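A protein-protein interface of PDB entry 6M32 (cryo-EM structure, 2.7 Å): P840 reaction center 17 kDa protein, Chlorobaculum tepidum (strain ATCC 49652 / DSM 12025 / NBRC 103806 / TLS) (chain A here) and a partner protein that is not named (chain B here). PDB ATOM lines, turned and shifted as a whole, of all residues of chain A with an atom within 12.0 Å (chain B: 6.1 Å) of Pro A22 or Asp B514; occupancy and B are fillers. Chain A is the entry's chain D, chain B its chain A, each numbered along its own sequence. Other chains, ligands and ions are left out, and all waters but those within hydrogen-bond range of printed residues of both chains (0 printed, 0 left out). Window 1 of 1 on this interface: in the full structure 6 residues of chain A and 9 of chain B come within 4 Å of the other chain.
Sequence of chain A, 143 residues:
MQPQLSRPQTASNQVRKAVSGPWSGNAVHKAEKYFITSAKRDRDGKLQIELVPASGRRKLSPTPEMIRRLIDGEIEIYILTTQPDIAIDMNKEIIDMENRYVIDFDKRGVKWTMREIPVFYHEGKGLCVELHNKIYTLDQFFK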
ATOM      1  N   SER A  20     -10.466  14.820   2.712  1.00  0.00           N
ATOM      2  CA  SER A  20     -11.642  15.683   2.725  1.00  0.00           C
ATOM      3  C   SER A  20     -12.433  15.514   4.018  1.00  0.00           C
ATOM      4  O   SER A  20     -11.947  14.921   4.981  1.00  0.00           O
ATOM      5  CB  SER A  20     -12.535  15.392   1.518  1.00  0.00           C
ATOM      6  OG  SER A  20     -12.902  14.024   1.471  1.00  0.00           O
ATOM      7  N   GLY A  21     -13.656  16.040   4.029  1.00  0.00           N
ATOM      8  CA  GLY A  21     -14.498  16.003   5.201  1.00  0.00           C
ATOM      9  C   GLY A  21     -14.861  14.594   5.618  1.00  0.00           C
ATOM     10  O   GLY A  21     -14.975  13.683   4.793  1.00  0.00           O
ATOM     11  N   PRO A  22     -15.036  14.387   6.927  1.00  0.00           N
ATOM     12  CA  PRO A  22     -15.401  13.050   7.419  1.00  0.00           C
ATOM     13  C   PRO A  22     -16.747  12.558   6.928  1.00  0.00           C
ATOM     14  O   PRO A  22     -16.977  11.344   6.932  1.00  0.00           O
ATOM     15  CB  PRO A  22     -15.407  13.224   8.944  1.00  0.00           C
ATOM     16  CG  PRO A  22     -14.560  14.420   9.196  1.00  0.00           C
ATOM     17  CD  PRO A  22     -14.770  15.327   8.027  1.00  0.00           C
ATOM     18  N   TRP A  23     -17.643  13.446   6.514  1.00  0.00           N
ATOM     19  CA  TRP A  23     -19.000  13.053   6.172  1.00  0.00           C
ATOM     20  C   TRP A  23     -19.169  12.670   4.708  1.00  0.00           C
ATOM     21  O   TRP A  23     -20.256  12.226   4.324  1.00  0.00           O
ATOM     22  CB  TRP A  23     -19.974  14.170   6.541  1.00  0.00           C
ATOM     23  CG  TRP A  23     -19.756  14.728   7.900  1.00  0.00           C
ATOM     24  CD1 TRP A  23     -20.328  14.300   9.061  1.00  0.00           C
ATOM     25  CD2 TRP A  23     -18.908  15.825   8.251  1.00  0.00           C
ATOM     26  NE1 TRP A  23     -19.888  15.061  10.114  1.00  0.00           N
ATOM     27  CE2 TRP A  23     -19.014  16.004   9.642  1.00  0.00           C
ATOM     28  CE3 TRP A  23     -18.069  16.672   7.524  1.00  0.00           C
ATOM     29  CZ2 TRP A  23     -18.314  16.994  10.319  1.00  0.00           C
ATOM     30  CZ3 TRP A  23     -17.375  17.652   8.198  1.00  0.00           C
ATOM     31  CH2 TRP A  23     -17.502  17.807   9.580  1.00  0.00           C
ATOM     32  N   SER A  24     -18.129  12.803   3.892  1.00  0.00           N
ATOM     33  CA  SER A  24     -18.156  12.349   2.508  1.00  0.00           C
ATOM     34  C   SER A  24     -17.472  10.994   2.412  1.00  0.00           C
ATOM     35  O   SER A  24     -16.473  10.745   3.093  1.00  0.00           O
ATOM     36  CB  SER A  24     -17.466  13.347   1.576  1.00  0.00           C
ATOM     37  OG  SER A  24     -16.079  13.425   1.852  1.00  0.00           O
ATOM     38  N   GLY A  25     -18.011  10.123   1.564  1.00  0.00           N
ATOM     39  CA  GLY A  25     -17.470   8.778   1.468  1.00  0.00           C
ATOM     40  C   GLY A  25     -17.729   7.999   2.742  1.00  0.00           C
ATOM     41  O   GLY A  25     -18.817   8.056   3.325  1.00  0.00           O
ATOM     42  N   ASN A  26     -16.718   7.263   3.189  1.00  0.00           N
ATOM     43  CA  ASN A  26     -16.799   6.500   4.425  1.00  0.00           C
ATOM     44  C   ASN A  26     -16.078   7.241   5.543  1.00  0.00           C
ATOM     45  O   ASN A  26     -15.011   7.825   5.332  1.00  0.00           O
ATOM     46  CB  ASN A  26     -16.200   5.105   4.252  1.00  0.00           C
ATOM     47  CG  ASN A  26     -16.677   4.136   5.312  1.00  0.00           C
ATOM     48  OD1 ASN A  26     -17.264   4.539   6.316  1.00  0.00           O
ATOM     49  ND2 ASN A  26     -16.430   2.850   5.095  1.00  0.00           N
ATOM     50  N   ALA A  27     -16.670   7.212   6.734  1.00  0.00           N
ATOM     51  CA  ALA A  27     -16.100   7.895   7.885  1.00  0.00           C
ATOM     52  C   ALA A  27     -14.913   7.157   8.489  1.00  0.00           C
ATOM     53  O   ALA A  27     -14.123   7.777   9.207  1.00  0.00           O
ATOM     54  CB  ALA A  27     -17.175   8.097   8.953  1.00  0.00           C
ATOM     55  N   VAL A  28     -14.773   5.859   8.222  1.00  0.00           N
ATOM     56  CA  VAL A  28     -13.658   5.101   8.778  1.00  0.00           C
ATOM     57  C   VAL A  28     -12.337   5.569   8.181  1.00  0.00           C
ATOM     58  O   VAL A  28     -11.346   5.748   8.897  1.00  0.00           O
ATOM     59  CB  VAL A  28     -13.877   3.593   8.553  1.00  0.00           C
ATOM     60  CG1 VAL A  28     -13.908   3.270   7.070  1.00  0.00           C
ATOM     61  CG2 VAL A  28     -12.789   2.796   9.242  1.00  0.00           C
ATOM     62  N   HIS A  29     -12.306   5.793   6.874  1.00  0.00           N
ATOM     63  CA  HIS A  29     -11.053   5.977   6.163  1.00  0.00           C
ATOM     64  C   HIS A  29     -10.759   7.453   5.926  1.00  0.00           C
ATOM     65  O   HIS A  29     -11.660   8.285   5.810  1.00  0.00           O
ATOM     66  CB  HIS A  29     -11.094   5.232   4.834  1.00  0.00           C
ATOM     67  CG  HIS A  29     -11.368   3.771   4.985  1.00  0.00           C
ATOM     68  ND1 HIS A  29     -12.230   3.088   4.154  1.00  0.00           N
ATOM     69  CD2 HIS A  29     -10.881   2.857   5.856  1.00  0.00           C
ATOM     70  CE1 HIS A  29     -12.267   1.818   4.512  1.00  0.00           C
ATOM     71  NE2 HIS A  29     -11.461   1.651   5.544  1.00  0.00           N
ATOM     72  N   LYS A  30      -9.468   7.767   5.857  1.00  0.00           N
ATOM     73  CA  LYS A  30      -9.011   9.114   5.555  1.00  0.00           C
ATOM     74  C   LYS A  30      -8.961   9.399   4.061  1.00  0.00           C
ATOM     75  O   LYS A  30      -8.796  10.561   3.674  1.00  0.00           O
ATOM     76  CB  LYS A  30      -7.628   9.352   6.169  1.00  0.00           C
ATOM     77  CG  LYS A  30      -7.436   8.697   7.528  1.00  0.00           C
ATOM     78  CD  LYS A  30      -8.405   9.264   8.557  1.00  0.00           C
ATOM     79  CE  LYS A  30      -8.220  10.763   8.735  1.00  0.00           C
ATOM     80  NZ  LYS A  30      -6.904  11.087   9.348  1.00  0.00           N
ATOM     81  N   ALA A  31      -9.096   8.376   3.221  1.00  0.00           N
ATOM     82  CA  ALA A  31      -9.142   8.553   1.776  1.00  0.00           C
ATOM     83  C   ALA A  31      -9.726   7.294   1.152  1.00  0.00           C
ATOM     84  O   ALA A  31      -9.937   6.282   1.825  1.00  0.00           O
ATOM     85  CB  ALA A  31      -7.760   8.863   1.200  1.00  0.00           C
ATOM     86  N   GLU A  32      -9.985   7.374  -0.150  1.00  0.00           N
ATOM     87  CA  GLU A  32     -10.614   6.275  -0.868  1.00  0.00           C
ATOM     88  C   GLU A  32      -9.719   5.042  -0.859  1.00  0.00           C
ATOM     89  O   GLU A  32      -8.556   5.101  -1.262  1.00  0.00           O
ATOM     90  CB  GLU A  32     -10.912   6.711  -2.303  1.00  0.00           C
ATOM     91  CG  GLU A  32     -11.614   5.681  -3.165  1.00  0.00           C
ATOM     92  CD  GLU A  32     -13.014   5.357  -2.683  1.00  0.00           C
ATOM     93  OE1 GLU A  32     -13.634   6.217  -2.023  1.00  0.00           O
ATOM     94  OE2 GLU A  32     -13.499   4.243  -2.976  1.00  0.00           O
ATOM     95  N   GLU A  76      -5.087   4.435  -1.460  1.00  0.00           N
ATOM     96  CA  GLU A  76      -4.378   3.364  -0.775  1.00  0.00           C
ATOM     97  C   GLU A  76      -4.899   2.028  -1.286  1.00  0.00           C
ATOM     98  O   GLU A  76      -6.096   1.881  -1.545  1.00  0.00           O
ATOM     99  CB  GLU A  76      -4.534   3.441   0.754  1.00  0.00           C
ATOM    100  CG  GLU A  76      -4.317   4.818   1.399  1.00  0.00           C
ATOM    101  CD  GLU A  76      -5.416   5.825   1.108  1.00  0.00           C
ATOM    102  OE1 GLU A  76      -5.296   6.979   1.571  1.00  0.00           O
ATOM    103  OE2 GLU A  76      -6.395   5.468   0.422  1.00  0.00           O
ATOM    104  N   ASP B 417     -18.515  21.116   9.723  1.00  0.00           N
ATOM    105  CA  ASP B 417     -17.154  21.434   9.295  1.00  0.00           C
ATOM    106  C   ASP B 417     -16.040  20.758  10.086  1.00  0.00           C
ATOM    107  O   ASP B 417     -14.967  20.554   9.512  1.00  0.00           O
ATOM    108  CB  ASP B 417     -16.938  22.952   9.332  1.00  0.00           C
ATOM    109  CG  ASP B 417     -15.798  23.406   8.447  1.00  0.00           C
ATOM    110  OD1 ASP B 417     -16.068  23.983   7.374  1.00  0.00           O
ATOM    111  OD2 ASP B 417     -14.629  23.213   8.831  1.00  0.00           O
ATOM    112  N   GLN B 418     -16.242  20.403  11.359  1.00  0.00           N
ATOM    113  CA  GLN B 418     -15.248  19.734  12.203  1.00  0.00           C
ATOM    114  C   GLN B 418     -14.079  20.633  12.609  1.00  0.00           C
ATOM    115  O   GLN B 418     -13.216  20.209  13.382  1.00  0.00           O
ATOM    116  CB  GLN B 418     -14.711  18.465  11.522  1.00  0.00           C
ATOM    117  CG  GLN B 418     -14.032  17.464  12.455  1.00  0.00           C
ATOM    118  CD  GLN B 418     -14.996  16.499  13.113  1.00  0.00           C
ATOM    119  OE1 GLN B 418     -16.191  16.765  13.210  1.00  0.00           O
ATOM    120  NE2 GLN B 418     -14.475  15.363  13.569  1.00  0.00           N
ATOM    121  N   HIS B 508     -22.041  10.837  15.134  1.00  0.00           N
ATOM    122  CA  HIS B 508     -21.487   9.788  14.290  1.00  0.00           C
ATOM    123  C   HIS B 508     -19.976   9.674  14.428  1.00  0.00           C
ATOM    124  O   HIS B 508     -19.450   8.579  14.640  1.00  0.00           O
ATOM    125  CB  HIS B 508     -21.853  10.053  12.827  1.00  0.00           C
ATOM    126  CG  HIS B 508     -21.511   8.932  11.900  1.00  0.00           C
ATOM    127  ND1 HIS B 508     -21.491   7.614  12.299  1.00  0.00           N
ATOM    128  CD2 HIS B 508     -21.175   8.934  10.588  1.00  0.00           C
ATOM    129  CE1 HIS B 508     -21.161   6.851  11.273  1.00  0.00           C
ATOM    130  NE2 HIS B 508     -20.962   7.627  10.223  1.00  0.00           N
ATOM    131  N   THR B 509     -19.267  10.790  14.303  1.00  0.00           N
ATOM    132  CA  THR B 509     -17.818  10.803  14.409  1.00  0.00           C
ATOM    133  C   THR B 509     -17.388  11.923  15.338  1.00  0.00           C
ATOM    134  O   THR B 509     -18.019  12.982  15.388  1.00  0.00           O
ATOM    135  CB  THR B 509     -17.143  10.996  13.046  1.00  0.00           C
ATOM    136  OG1 THR B 509     -17.538  12.255  12.491  1.00  0.00           O
ATOM    137  CG2 THR B 509     -17.531   9.884  12.090  1.00  0.00           C
ATOM    138  N   SER B 510     -16.315  11.682  16.056  1.00  0.00           N
ATOM    139  CA  SER B 510     -15.612  12.626  16.895  1.00  0.00           C
ATOM    140  C   SER B 510     -14.199  12.810  16.359  1.00  0.00           C
ATOM    141  O   SER B 510     -13.697  11.945  15.635  1.00  0.00           O
ATOM    142  CB  SER B 510     -15.564  12.126  18.344  1.00  0.00           C
ATOM    143  OG  SER B 510     -14.794  12.964  19.183  1.00  0.00           O
ATOM    144  N   PRO B 511     -13.539  13.931  16.659  1.00  0.00           N
ATOM    145  CA  PRO B 511     -12.157  14.098  16.187  1.00  0.00           C
ATOM    146  C   PRO B 511     -11.242  12.959  16.590  1.00  0.00           C
ATOM    147  O   PRO B 511     -10.365  12.575  15.810  1.00  0.00           O
ATOM    148  CB  PRO B 511     -11.736  15.423  16.829  1.00  0.00           C
ATOM    149  CG  PRO B 511     -12.996  16.184  16.929  1.00  0.00           C
ATOM    150  CD  PRO B 511     -14.071  15.178  17.231  1.00  0.00           C
ATOM    151  N   LEU B 512     -11.427  12.403  17.788  1.00  0.00           N
ATOM    152  CA  LEU B 512     -10.609  11.272  18.211  1.00  0.00           C
ATOM    153  C   LEU B 512     -11.032   9.987  17.513  1.00  0.00           C
ATOM    154  O   LEU B 512     -10.186   9.160  17.154  1.00  0.00           O
ATOM    155  CB  LEU B 512     -10.693  11.111  19.725  1.00  0.00           C
ATOM    156  CG  LEU B 512      -9.864   9.976  20.309  1.00  0.00           C
ATOM    157  CD1 LEU B 512      -8.390  10.243  20.076  1.00  0.00           C
ATOM    158  CD2 LEU B 512     -10.155   9.849  21.781  1.00  0.00           C
ATOM    159  N   TRP B 513     -12.336   9.791  17.325  1.00  0.00           N
ATOM    160  CA  TRP B 513     -12.806   8.571  16.683  1.00  0.00           C
ATOM    161  C   TRP B 513     -12.480   8.571  15.198  1.00  0.00           C
ATOM    162  O   TRP B 513     -12.197   7.514  14.626  1.00  0.00           O
ATOM    163  CB  TRP B 513     -14.302   8.410  16.931  1.00  0.00           C
ATOM    164  CG  TRP B 513     -14.579   8.155  18.375  1.00  0.00           C
ATOM    165  CD1 TRP B 513     -14.945   9.079  19.304  1.00  0.00           C
ATOM    166  CD2 TRP B 513     -14.498   6.905  19.066  1.00  0.00           C
ATOM    167  NE1 TRP B 513     -15.097   8.488  20.530  1.00  0.00           N
ATOM    168  CE2 TRP B 513     -14.831   7.150  20.411  1.00  0.00           C
ATOM    169  CE3 TRP B 513     -14.184   5.604  18.679  1.00  0.00           C
ATOM    170  CZ2 TRP B 513     -14.855   6.144  21.369  1.00  0.00           C
ATOM    171  CZ3 TRP B 513     -14.207   4.604  19.636  1.00  0.00           C
ATOM    172  CH2 TRP B 513     -14.542   4.880  20.963  1.00  0.00           C
ATOM    173  N   ASP B 514     -12.514   9.736  14.556  1.00  0.00           N
ATOM    174  CA  ASP B 514     -11.959   9.847  13.216  1.00  0.00           C
ATOM    175  C   ASP B 514     -10.442   9.937  13.230  1.00  0.00           C
ATOM    176  O   ASP B 514      -9.806   9.645  12.209  1.00  0.00           O
ATOM    177  CB  ASP B 514     -12.533  11.063  12.486  1.00  0.00           C
ATOM    178  CG  ASP B 514     -12.077  11.142  11.037  1.00  0.00           C
ATOM    179  OD1 ASP B 514     -12.038  10.097  10.350  1.00  0.00           O
ATOM    180  OD2 ASP B 514     -11.753  12.257  10.584  1.00  0.00           O
ATOM    181  N   ASP B 515      -9.841  10.333  14.354  1.00  0.00           N
ATOM    182  CA  ASP B 515      -8.388  10.245  14.455  1.00  0.00           C
ATOM    183  C   ASP B 515      -7.934   8.810  14.268  1.00  0.00           C
ATOM    184  O   ASP B 515      -6.934   8.550  13.589  1.00  0.00           O
ATOM    185  CB  ASP B 515      -7.898  10.792  15.798  1.00  0.00           C
ATOM    186  CG  ASP B 515      -6.380  10.810  15.909  1.00  0.00           C
ATOM    187  OD1 ASP B 515      -5.703  10.416  14.937  1.00  0.00           O
ATOM    188  OD2 ASP B 515      -5.856  11.234  16.958  1.00  0.00           O
ATOM    189  N   LEU B 516      -8.656   7.867  14.866  1.00  0.00           N
ATOM    190  CA  LEU B 516      -8.478   6.467  14.533  1.00  0.00           C
ATOM    191  C   LEU B 516      -9.460   6.096  13.419  1.00  0.00           C
ATOM    192  O   LEU B 516     -10.158   6.948  12.864  1.00  0.00           O
ATOM    193  CB  LEU B 516      -8.692   5.582  15.758  1.00  0.00           C
ATOM    194  CG  LEU B 516      -7.638   5.817  16.847  1.00  0.00           C
ATOM    195  CD1 LEU B 516      -8.005   5.010  18.090  1.00  0.00           C
ATOM    196  CD2 LEU B 516      -6.183   5.639  16.443  1.00  0.00           C
ATOM    197  N   GLY B 517      -9.491   4.817  13.063  1.00  0.00           N
ATOM    198  CA  GLY B 517     -10.524   4.368  12.152  1.00  0.00           C
ATOM    199  C   GLY B 517     -11.700   3.743  12.876  1.00  0.00           C
ATOM    200  O   GLY B 517     -11.673   2.541  13.153  1.00  0.00           O
ATOM    201  N   LEU B 518     -12.752   4.515  13.147  1.00  0.00           N
ATOM    202  CA  LEU B 518     -13.816   4.016  14.008  1.00  0.00           C
ATOM    203  C   LEU B 518     -15.142   4.697  13.684  1.00  0.00           C
ATOM    204  O   LEU B 518     -15.184   5.718  12.993  1.00  0.00           O
ATOM    205  CB  LEU B 518     -13.459   4.204  15.490  1.00  0.00           C
ATOM    206  CG  LEU B 518     -12.411   3.217  16.019  1.00  0.00           C
ATOM    207  CD1 LEU B 518     -11.823   3.640  17.338  1.00  0.00           C
ATOM    208  CD2 LEU B 518     -13.000   1.826  16.116  1.00  0.00           C
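O of Ala A27 sits close to OD1 of Asp B514 (3.3 Å).
The side-chain amide oxygen of Asn A26 sits close to the backbone NH of Val A28, at 3.4 Å.
Pro A22 touches Asp B514 (CG to OD2, 3.8 Å). Asp B417 touches Trp A23. Trp A23 touches Gln B418. CB of Ala A27 touches CG2 of Thr B509, 3.6 Å away. O of Val A28 touches CA of Gly B517, at 3.6 Å. O of Asp B514 touches CD of Lys A30, at 3.9 Å.
Pro A22 touches one residue of chain B. Of the printed residues of chain B, Trp A23 touches Asp B417 (3.3 Å) and Gln B418 (3.4 Å). Of the printed residues of chain B, Val A28 touches Gly B517 (3.6 Å). Of the printed residues of chain B, Lys A30 touches Asp B514 (3.9 Å). Of the printed residues of chain A, Asp B417 touches Trp A23 (3.3 Å). Thr B509 touches just one residue of chain A: Ala A27 (3.6 Å). No residue of chain A comes within 4 Å of Ser B510. No residue of chain A comes within 4 Å of Pro B511. No residue of chain A comes within 4 Å of Leu B512. Asp B514 touches just these residues of chain A: Pro A22, Ala A27 and Lys A30. No residue of chain A comes within 4 Å of Asp B515. Gly B517 touches one residue of chain A. The nearest printed residue of chain A that does not touch Asp B417 is Pro A22 (5.4 Å).
Along chain B the printed residues that touch a printed residue of chain A span positions 417 to 517. Hydrophobic or aromatic side chains of chain A within 4 Å of the printed part of chain B: Pro A22, Trp A23, Ala A27 and Val A28. Among the printed residues, no Asp or Glu carboxylate lies within 4 Å of a Lys or Arg side-chain nitrogen of the other chain.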
